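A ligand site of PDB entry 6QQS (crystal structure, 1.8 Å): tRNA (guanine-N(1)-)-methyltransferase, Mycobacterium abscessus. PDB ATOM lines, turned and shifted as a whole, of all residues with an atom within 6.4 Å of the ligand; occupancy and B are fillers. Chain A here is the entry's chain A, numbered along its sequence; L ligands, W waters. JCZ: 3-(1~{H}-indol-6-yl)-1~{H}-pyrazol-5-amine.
O of Gly 136 lies within hydrogen-bond range of N01 of the ligand. N of Leu 140 lies within hydrogen-bond range of N04 of the ligand, 3.0 Å away. OG of Ser 134 is in hydrogen-bond range of N01 of the ligand, 3.1 Å away. The backbone carbonyl oxygen (O) of Tyr 138 sits at hydrogen-bond distance from a nitrogen (N03) of the ligand (2.8 Å).
The side-chain hydroxyl (OH) of Tyr 138 lies within hydrogen-bond range of the backbone carbonyl oxygen (O) of Ile 135 (3.2 Å). The backbone NH of Gly 143 lies within hydrogen-bond range of the backbone carbonyl oxygen of Gly 111 (2.9 Å). N of Thr 86 sits at hydrogen-bond distance from O of Val 133, at 2.9 Å. The side-chain hydroxyl (OG) of Ser 134 is in hydrogen-bond range of the backbone carbonyl oxygen (O) of Gly 136. The side-chain carboxylate of Glu 144 lies within salt-bridge range of the guanidinium group of Arg 112, 2.9 Å away. The side-chain hydroxyl (OG1) of Thr 86 lies close to the backbone NH (N) of Ala 88, at 3.1 Å.
A nitrogen (N01) of the ligand sits close to the backbone NH (N) of Ile 135 (3.2 Å). Merely in contact with the ligand: Tyr 113 (3.1 Å), Gly 111 (3.3 Å), Pro 85 (3.4 Å), Gly 143 (3.4 Å), Pro 87 (3.5 Å), Asn 141 (3.5 Å), Gly 142 (3.5 Å), Thr 86 (3.6 Å), Arg 112 (3.7 Å) and Val 139 (3.8 Å). 15 residues have an atom within 4 Å of the ligand: Pro 85, Thr 86, Pro 87, Gly 111, Arg 112, Tyr 113, Ser 134, Ile 135, Gly 136, Tyr 138, Val 139, Leu 140, Asn 141, Gly 142 and Gly 143. The nearest printed residue that does not touch the ligand is Gly 115 (4.3 Å).
Water W1 bridges O of Leu 140 (2.7 Å) and N12 of the ligand (2.9 Å).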
ATOM      1  N   PRO A  85      -8.046  16.739  -3.557  1.00  0.00           N
ATOM      2  CA  PRO A  85      -7.604  17.150  -2.222  1.00  0.00           C
ATOM      3  C   PRO A  85      -8.306  18.426  -1.777  1.00  0.00           C
ATOM      4  O   PRO A  85      -8.510  19.334  -2.596  1.00  0.00           O
ATOM      5  CB  PRO A  85      -6.097  17.399  -2.403  1.00  0.00           C
ATOM      6  CG  PRO A  85      -5.707  16.472  -3.531  1.00  0.00           C
ATOM      7  CD  PRO A  85      -6.912  16.539  -4.477  1.00  0.00           C
ATOM      8  N   THR A  86      -8.700  18.483  -0.524  1.00  0.00           N
ATOM      9  CA  THR A  86      -9.389  19.648   0.033  1.00  0.00           C
ATOM     10  C   THR A  86      -9.348  19.545   1.551  1.00  0.00           C
ATOM     11  O   THR A  86      -9.424  18.436   2.095  1.00  0.00           O
ATOM     12  CB  THR A  86     -10.854  19.739  -0.468  1.00  0.00           C
ATOM     13  OG1 THR A  86     -11.587  20.661   0.355  1.00  0.00           O
ATOM     14  CG2 THR A  86     -11.522  18.384  -0.408  1.00  0.00           C
ATOM     15  N   PRO A  87      -9.213  20.686   2.251  1.00  0.00           N
ATOM     16  CA  PRO A  87      -9.218  20.645   3.717  1.00  0.00           C
ATOM     17  C   PRO A  87     -10.539  20.148   4.257  1.00  0.00           C
ATOM     18  O   PRO A  87     -10.615  19.762   5.431  1.00  0.00           O
ATOM     19  CB  PRO A  87      -9.007  22.107   4.135  1.00  0.00           C
ATOM     20  CG  PRO A  87      -8.453  22.773   2.914  1.00  0.00           C
ATOM     21  CD  PRO A  87      -9.049  22.062   1.750  1.00  0.00           C
ATOM     22  N   ALA A  88     -11.565  20.189   3.416  1.00  0.00           N
ATOM     23  CA  ALA A  88     -12.906  19.788   3.793  1.00  0.00           C
ATOM     24  C   ALA A  88     -13.213  18.350   3.396  1.00  0.00           C
ATOM     25  O   ALA A  88     -14.370  17.946   3.346  1.00  0.00           O
ATOM     26  CB  ALA A  88     -13.940  20.740   3.164  1.00  0.00           C
ATOM     27  N   CYS A 110      -5.812  19.145  -8.559  1.00  0.00           N
ATOM     28  CA  CYS A 110      -5.223  20.030  -7.552  1.00  0.00           C
ATOM     29  C   CYS A 110      -5.822  21.424  -7.639  1.00  0.00           C
ATOM     30  O   CYS A 110      -5.629  22.115  -8.628  1.00  0.00           O
ATOM     31  CB  CYS A 110      -3.718  20.137  -7.734  1.00  0.00           C
ATOM     32  SG  CYS A 110      -2.870  18.583  -7.538  1.00  0.00           S
ATOM     33  N   GLY A 111      -6.515  21.827  -6.588  1.00  0.00           N
ATOM     34  CA  GLY A 111      -7.047  23.171  -6.523  1.00  0.00           C
ATOM     35  C   GLY A 111      -6.062  24.203  -5.999  1.00  0.00           C
ATOM     36  O   GLY A 111      -5.036  23.865  -5.422  1.00  0.00           O
ATOM     37  N   ARG A 112      -6.380  25.469  -6.239  1.00  0.00           N
ATOM     38  CA  ARG A 112      -5.666  26.603  -5.635  1.00  0.00           C
ATOM     39  C   ARG A 112      -6.700  27.651  -5.211  1.00  0.00           C
ATOM     40  O   ARG A 112      -7.895  27.395  -5.267  1.00  0.00           O
ATOM     41  CB  ARG A 112      -4.644  27.197  -6.616  1.00  0.00           C
ATOM     42  CG  ARG A 112      -3.322  26.425  -6.710  1.00  0.00           C
ATOM     43  CD  ARG A 112      -2.313  26.923  -5.665  1.00  0.00           C
ATOM     44  NE  ARG A 112      -1.326  25.906  -5.328  1.00  0.00           N
ATOM     45  CZ  ARG A 112      -0.226  26.157  -4.632  1.00  0.00           C
ATOM     46  NH1 ARG A 112       0.041  27.396  -4.216  1.00  0.00           N
ATOM     47  NH2 ARG A 112       0.627  25.166  -4.363  1.00  0.00           N
ATOM     48  N   TYR A 113      -6.230  28.826  -4.796  1.00  0.00           N
ATOM     49  CA  TYR A 113      -7.114  29.886  -4.302  1.00  0.00           C
ATOM     50  C   TYR A 113      -8.057  29.354  -3.232  1.00  0.00           C
ATOM     51  O   TYR A 113      -7.619  28.694  -2.291  1.00  0.00           O
ATOM     52  CB  TYR A 113      -7.904  30.506  -5.460  1.00  0.00           C
ATOM     53  CG  TYR A 113      -7.036  30.895  -6.646  1.00  0.00           C
ATOM     54  CD1 TYR A 113      -6.397  32.123  -6.693  1.00  0.00           C
ATOM     55  CD2 TYR A 113      -6.844  30.027  -7.704  1.00  0.00           C
ATOM     56  CE1 TYR A 113      -5.603  32.486  -7.764  1.00  0.00           C
ATOM     57  CE2 TYR A 113      -6.056  30.361  -8.787  1.00  0.00           C
ATOM     58  CZ  TYR A 113      -5.435  31.591  -8.812  1.00  0.00           C
ATOM     59  OH  TYR A 113      -4.645  31.934  -9.885  1.00  0.00           O
ATOM     60  N   GLU A 114      -9.354  29.588  -3.373  1.00  0.00           N
ATOM     61  CA  GLU A 114     -10.312  29.075  -2.391  1.00  0.00           C
ATOM     62  C   GLU A 114     -11.005  27.785  -2.827  1.00  0.00           C
ATOM     63  O   GLU A 114     -12.060  27.438  -2.297  1.00  0.00           O
ATOM     64  CB  GLU A 114     -11.363  30.142  -2.064  1.00  0.00           C
ATOM     65  CG  GLU A 114     -10.770  31.452  -1.538  1.00  0.00           C
ATOM     66  CD  GLU A 114      -9.709  31.239  -0.462  1.00  0.00           C
ATOM     67  OE1 GLU A 114      -8.617  31.837  -0.573  1.00  0.00           O
ATOM     68  OE2 GLU A 114      -9.968  30.469   0.496  1.00  0.00           O
ATOM     69  N   GLY A 115     -10.424  27.068  -3.773  1.00  0.00           N
ATOM     70  CA  GLY A 115     -10.951  25.768  -4.153  1.00  0.00           C
ATOM     71  C   GLY A 115     -11.636  25.754  -5.508  1.00  0.00           C
ATOM     72  O   GLY A 115     -11.625  26.742  -6.218  1.00  0.00           O
ATOM     73  N   ILE A 116     -12.236  24.617  -5.860  1.00  0.00           N
ATOM     74  CA  ILE A 116     -12.855  24.427  -7.173  1.00  0.00           C
ATOM     75  C   ILE A 116     -14.364  24.528  -7.066  1.00  0.00           C
ATOM     76  O   ILE A 116     -14.934  23.983  -6.117  1.00  0.00           O
ATOM     77  CB  ILE A 116     -12.487  23.041  -7.741  1.00  0.00           C
ATOM     78  CG1 ILE A 116     -10.971  22.850  -7.725  1.00  0.00           C
ATOM     79  CG2 ILE A 116     -13.082  22.853  -9.137  1.00  0.00           C
ATOM     80  CD1 ILE A 116     -10.529  21.463  -8.138  1.00  0.00           C
ATOM     81  N   VAL A 133     -10.746  14.430  -0.471  1.00  0.00           N
ATOM     82  CA  VAL A 133     -10.012  13.960   0.702  1.00  0.00           C
ATOM     83  C   VAL A 133      -9.063  14.997   1.260  1.00  0.00           C
ATOM     84  O   VAL A 133      -8.531  15.829   0.517  1.00  0.00           O
ATOM     85  CB  VAL A 133      -9.186  12.674   0.417  1.00  0.00           C
ATOM     86  CG1 VAL A 133     -10.105  11.495   0.098  1.00  0.00           C
ATOM     87  CG2 VAL A 133      -8.155  12.900  -0.713  1.00  0.00           C
ATOM     88  N   SER A 134      -8.897  14.906   2.568  1.00  0.00           N
ATOM     89  CA  SER A 134      -7.954  15.727   3.331  1.00  0.00           C
ATOM     90  C   SER A 134      -6.800  14.846   3.805  1.00  0.00           C
ATOM     91  O   SER A 134      -7.021  13.717   4.249  1.00  0.00           O
ATOM     92  CB  SER A 134      -8.647  16.365   4.531  1.00  0.00           C
ATOM     93  OG  SER A 134      -7.699  16.943   5.436  1.00  0.00           O
ATOM     94  N   ILE A 135      -5.575  15.358   3.747  1.00  0.00           N
ATOM     95  CA  ILE A 135      -4.443  14.581   4.242  1.00  0.00           C
ATOM     96  C   ILE A 135      -4.057  14.903   5.685  1.00  0.00           C
ATOM     97  O   ILE A 135      -3.126  14.308   6.219  1.00  0.00           O
ATOM     98  CB  ILE A 135      -3.183  14.763   3.371  1.00  0.00           C
ATOM     99  CG1 ILE A 135      -2.708  16.219   3.355  1.00  0.00           C
ATOM    100  CG2 ILE A 135      -3.423  14.192   1.958  1.00  0.00           C
ATOM    101  CD1 ILE A 135      -1.243  16.362   2.887  1.00  0.00           C
ATOM    102  N   GLY A 136      -4.775  15.834   6.316  1.00  0.00           N
ATOM    103  CA  GLY A 136      -4.450  16.191   7.696  1.00  0.00           C
ATOM    104  C   GLY A 136      -5.153  17.480   8.092  1.00  0.00           C
ATOM    105  O   GLY A 136      -5.664  18.208   7.243  1.00  0.00           O
ATOM    106  N   ASP A 137      -5.163  17.755   9.392  1.00  0.00           N
ATOM    107  CA  ASP A 137      -5.898  18.910   9.901  1.00  0.00           C
ATOM    108  C   ASP A 137      -5.064  20.183   9.912  1.00  0.00           C
ATOM    109  O   ASP A 137      -4.804  20.764  10.962  1.00  0.00           O
ATOM    110  CB  ASP A 137      -6.414  18.633  11.299  1.00  0.00           C
ATOM    111  CG  ASP A 137      -7.542  17.621  11.300  1.00  0.00           C
ATOM    112  OD1 ASP A 137      -8.169  17.427  10.229  1.00  0.00           O
ATOM    113  OD2 ASP A 137      -7.804  17.028  12.362  1.00  0.00           O
ATOM    114  N   TYR A 138      -4.657  20.608   8.725  1.00  0.00           N
ATOM    115  CA  TYR A 138      -3.887  21.820   8.576  1.00  0.00           C
ATOM    116  C   TYR A 138      -4.264  22.295   7.194  1.00  0.00           C
ATOM    117  O   TYR A 138      -4.749  21.503   6.386  1.00  0.00           O
ATOM    118  CB  TYR A 138      -2.372  21.562   8.698  1.00  0.00           C
ATOM    119  CG  TYR A 138      -1.967  20.255   8.072  1.00  0.00           C
ATOM    120  CD1 TYR A 138      -1.871  20.113   6.696  1.00  0.00           C
ATOM    121  CD2 TYR A 138      -1.728  19.129   8.862  1.00  0.00           C
ATOM    122  CE1 TYR A 138      -1.528  18.905   6.113  1.00  0.00           C
ATOM    123  CE2 TYR A 138      -1.392  17.931   8.301  1.00  0.00           C
ATOM    124  CZ  TYR A 138      -1.292  17.820   6.916  1.00  0.00           C
ATOM    125  OH  TYR A 138      -0.975  16.625   6.357  1.00  0.00           O
ATOM    126  N   VAL A 139      -4.033  23.574   6.921  1.00  0.00           N
ATOM    127  CA  VAL A 139      -4.385  24.151   5.635  1.00  0.00           C
ATOM    128  C   VAL A 139      -3.143  24.446   4.795  1.00  0.00           C
ATOM    129  O   VAL A 139      -2.206  25.084   5.262  1.00  0.00           O
ATOM    130  CB  VAL A 139      -5.205  25.451   5.850  1.00  0.00           C
ATOM    131  CG1 VAL A 139      -5.489  26.151   4.528  1.00  0.00           C
ATOM    132  CG2 VAL A 139      -6.499  25.141   6.583  1.00  0.00           C
ATOM    133  N   LEU A 140      -3.170  23.970   3.563  1.00  0.00           N
ATOM    134  CA  LEU A 140      -2.112  24.213   2.582  1.00  0.00           C
ATOM    135  C   LEU A 140      -2.541  25.368   1.659  1.00  0.00           C
ATOM    136  O   LEU A 140      -3.671  25.824   1.743  1.00  0.00           O
ATOM    137  CB  LEU A 140      -1.861  22.943   1.771  1.00  0.00           C
ATOM    138  CG  LEU A 140      -1.430  21.723   2.599  1.00  0.00           C
ATOM    139  CD1 LEU A 140      -1.524  20.460   1.775  1.00  0.00           C
ATOM    140  CD2 LEU A 140      -0.030  21.914   3.126  1.00  0.00           C
ATOM    141  N   ASN A 141      -1.657  25.806   0.777  1.00  0.00           N
ATOM    142  CA  ASN A 141      -2.013  26.833  -0.233  1.00  0.00           C
ATOM    143  C   ASN A 141      -2.775  26.242  -1.415  1.00  0.00           C
ATOM    144  O   ASN A 141      -3.440  26.969  -2.172  1.00  0.00           O
ATOM    145  CB  ASN A 141      -0.751  27.521  -0.753  1.00  0.00           C
ATOM    146  CG  ASN A 141      -0.160  28.487   0.240  1.00  0.00           C
ATOM    147  OD1 ASN A 141      -0.872  29.125   1.009  1.00  0.00           O
ATOM    148  ND2 ASN A 141       1.169  28.603   0.224  1.00  0.00           N
ATOM    149  N   GLY A 142      -2.674  24.937  -1.593  1.00  0.00           N
ATOM    150  CA  GLY A 142      -3.281  24.278  -2.743  1.00  0.00           C
ATOM    151  C   GLY A 142      -3.126  22.773  -2.649  1.00  0.00           C
ATOM    152  O   GLY A 142      -2.541  22.260  -1.689  1.00  0.00           O
ATOM    153  N   GLY A 143      -3.646  22.059  -3.639  1.00  0.00           N
ATOM    154  CA  GLY A 143      -3.670  20.607  -3.587  1.00  0.00           C
ATOM    155  C   GLY A 143      -2.369  19.906  -3.925  1.00  0.00           C
ATOM    156  O   GLY A 143      -2.259  18.697  -3.725  1.00  0.00           O
ATOM    157  N   GLU A 144      -1.376  20.628  -4.451  1.00  0.00           N
ATOM    158  CA  GLU A 144      -0.185  19.976  -4.958  1.00  0.00           C
ATOM    159  C   GLU A 144       0.601  19.189  -3.894  1.00  0.00           C
ATOM    160  O   GLU A 144       1.015  18.039  -4.135  1.00  0.00           O
ATOM    161  CB  GLU A 144       0.729  20.995  -5.637  1.00  0.00           C
ATOM    162  CG  GLU A 144       0.163  21.518  -6.960  1.00  0.00           C
ATOM    163  CD  GLU A 144      -0.900  22.609  -6.812  1.00  0.00           C
ATOM    164  OE1 GLU A 144      -1.116  23.079  -5.662  1.00  0.00           O
ATOM    165  OE2 GLU A 144      -1.502  22.997  -7.841  1.00  0.00           O
ATOM    166  N   ALA A 146      -0.550  17.910  -1.234  1.00  0.00           N
ATOM    167  CA  ALA A 146      -1.391  16.768  -0.883  1.00  0.00           C
ATOM    168  C   ALA A 146      -1.305  15.683  -1.939  1.00  0.00           C
ATOM    169  O   ALA A 146      -1.313  14.497  -1.627  1.00  0.00           O
ATOM    170  CB  ALA A 146      -2.837  17.219  -0.693  1.00  0.00           C
HETATM  171  C10 JCZ L   1      -6.901  24.520  -2.729  1.00  0.00           C
HETATM  172  N12 JCZ L   1      -6.311  25.469  -0.821  1.00  0.00           N
HETATM  173  C13 JCZ L   1      -6.588  22.059  -1.896  1.00  0.00           C
HETATM  174  C15 JCZ L   1      -5.812  19.879   1.940  1.00  0.00           C
HETATM  175  N01 JCZ L   1      -5.442  18.507   4.039  1.00  0.00           N
HETATM  176  C02 JCZ L   1      -5.393  19.706   3.261  1.00  0.00           C
HETATM  177  N03 JCZ L   1      -4.909  20.887   3.706  1.00  0.00           N
HETATM  178  N04 JCZ L   1      -5.009  21.789   2.717  1.00  0.00           N
HETATM  179  C05 JCZ L   1      -5.526  21.201   1.646  1.00  0.00           C
HETATM  180  C06 JCZ L   1      -5.846  21.954   0.391  1.00  0.00           C
HETATM  181  C07 JCZ L   1      -5.859  23.340   0.499  1.00  0.00           C
HETATM  182  C08 JCZ L   1      -6.226  24.113  -0.640  1.00  0.00           C
HETATM  183  C09 JCZ L   1      -6.588  23.476  -1.818  1.00  0.00           C
HETATM  184  C11 JCZ L   1      -6.710  25.727  -2.078  1.00  0.00           C
HETATM  185  C14 JCZ L   1      -6.233  21.291  -0.796  1.00  0.00           C
HETATM  186  O   HOH W   1      -5.605  27.549   1.043  1.00  0.00           O
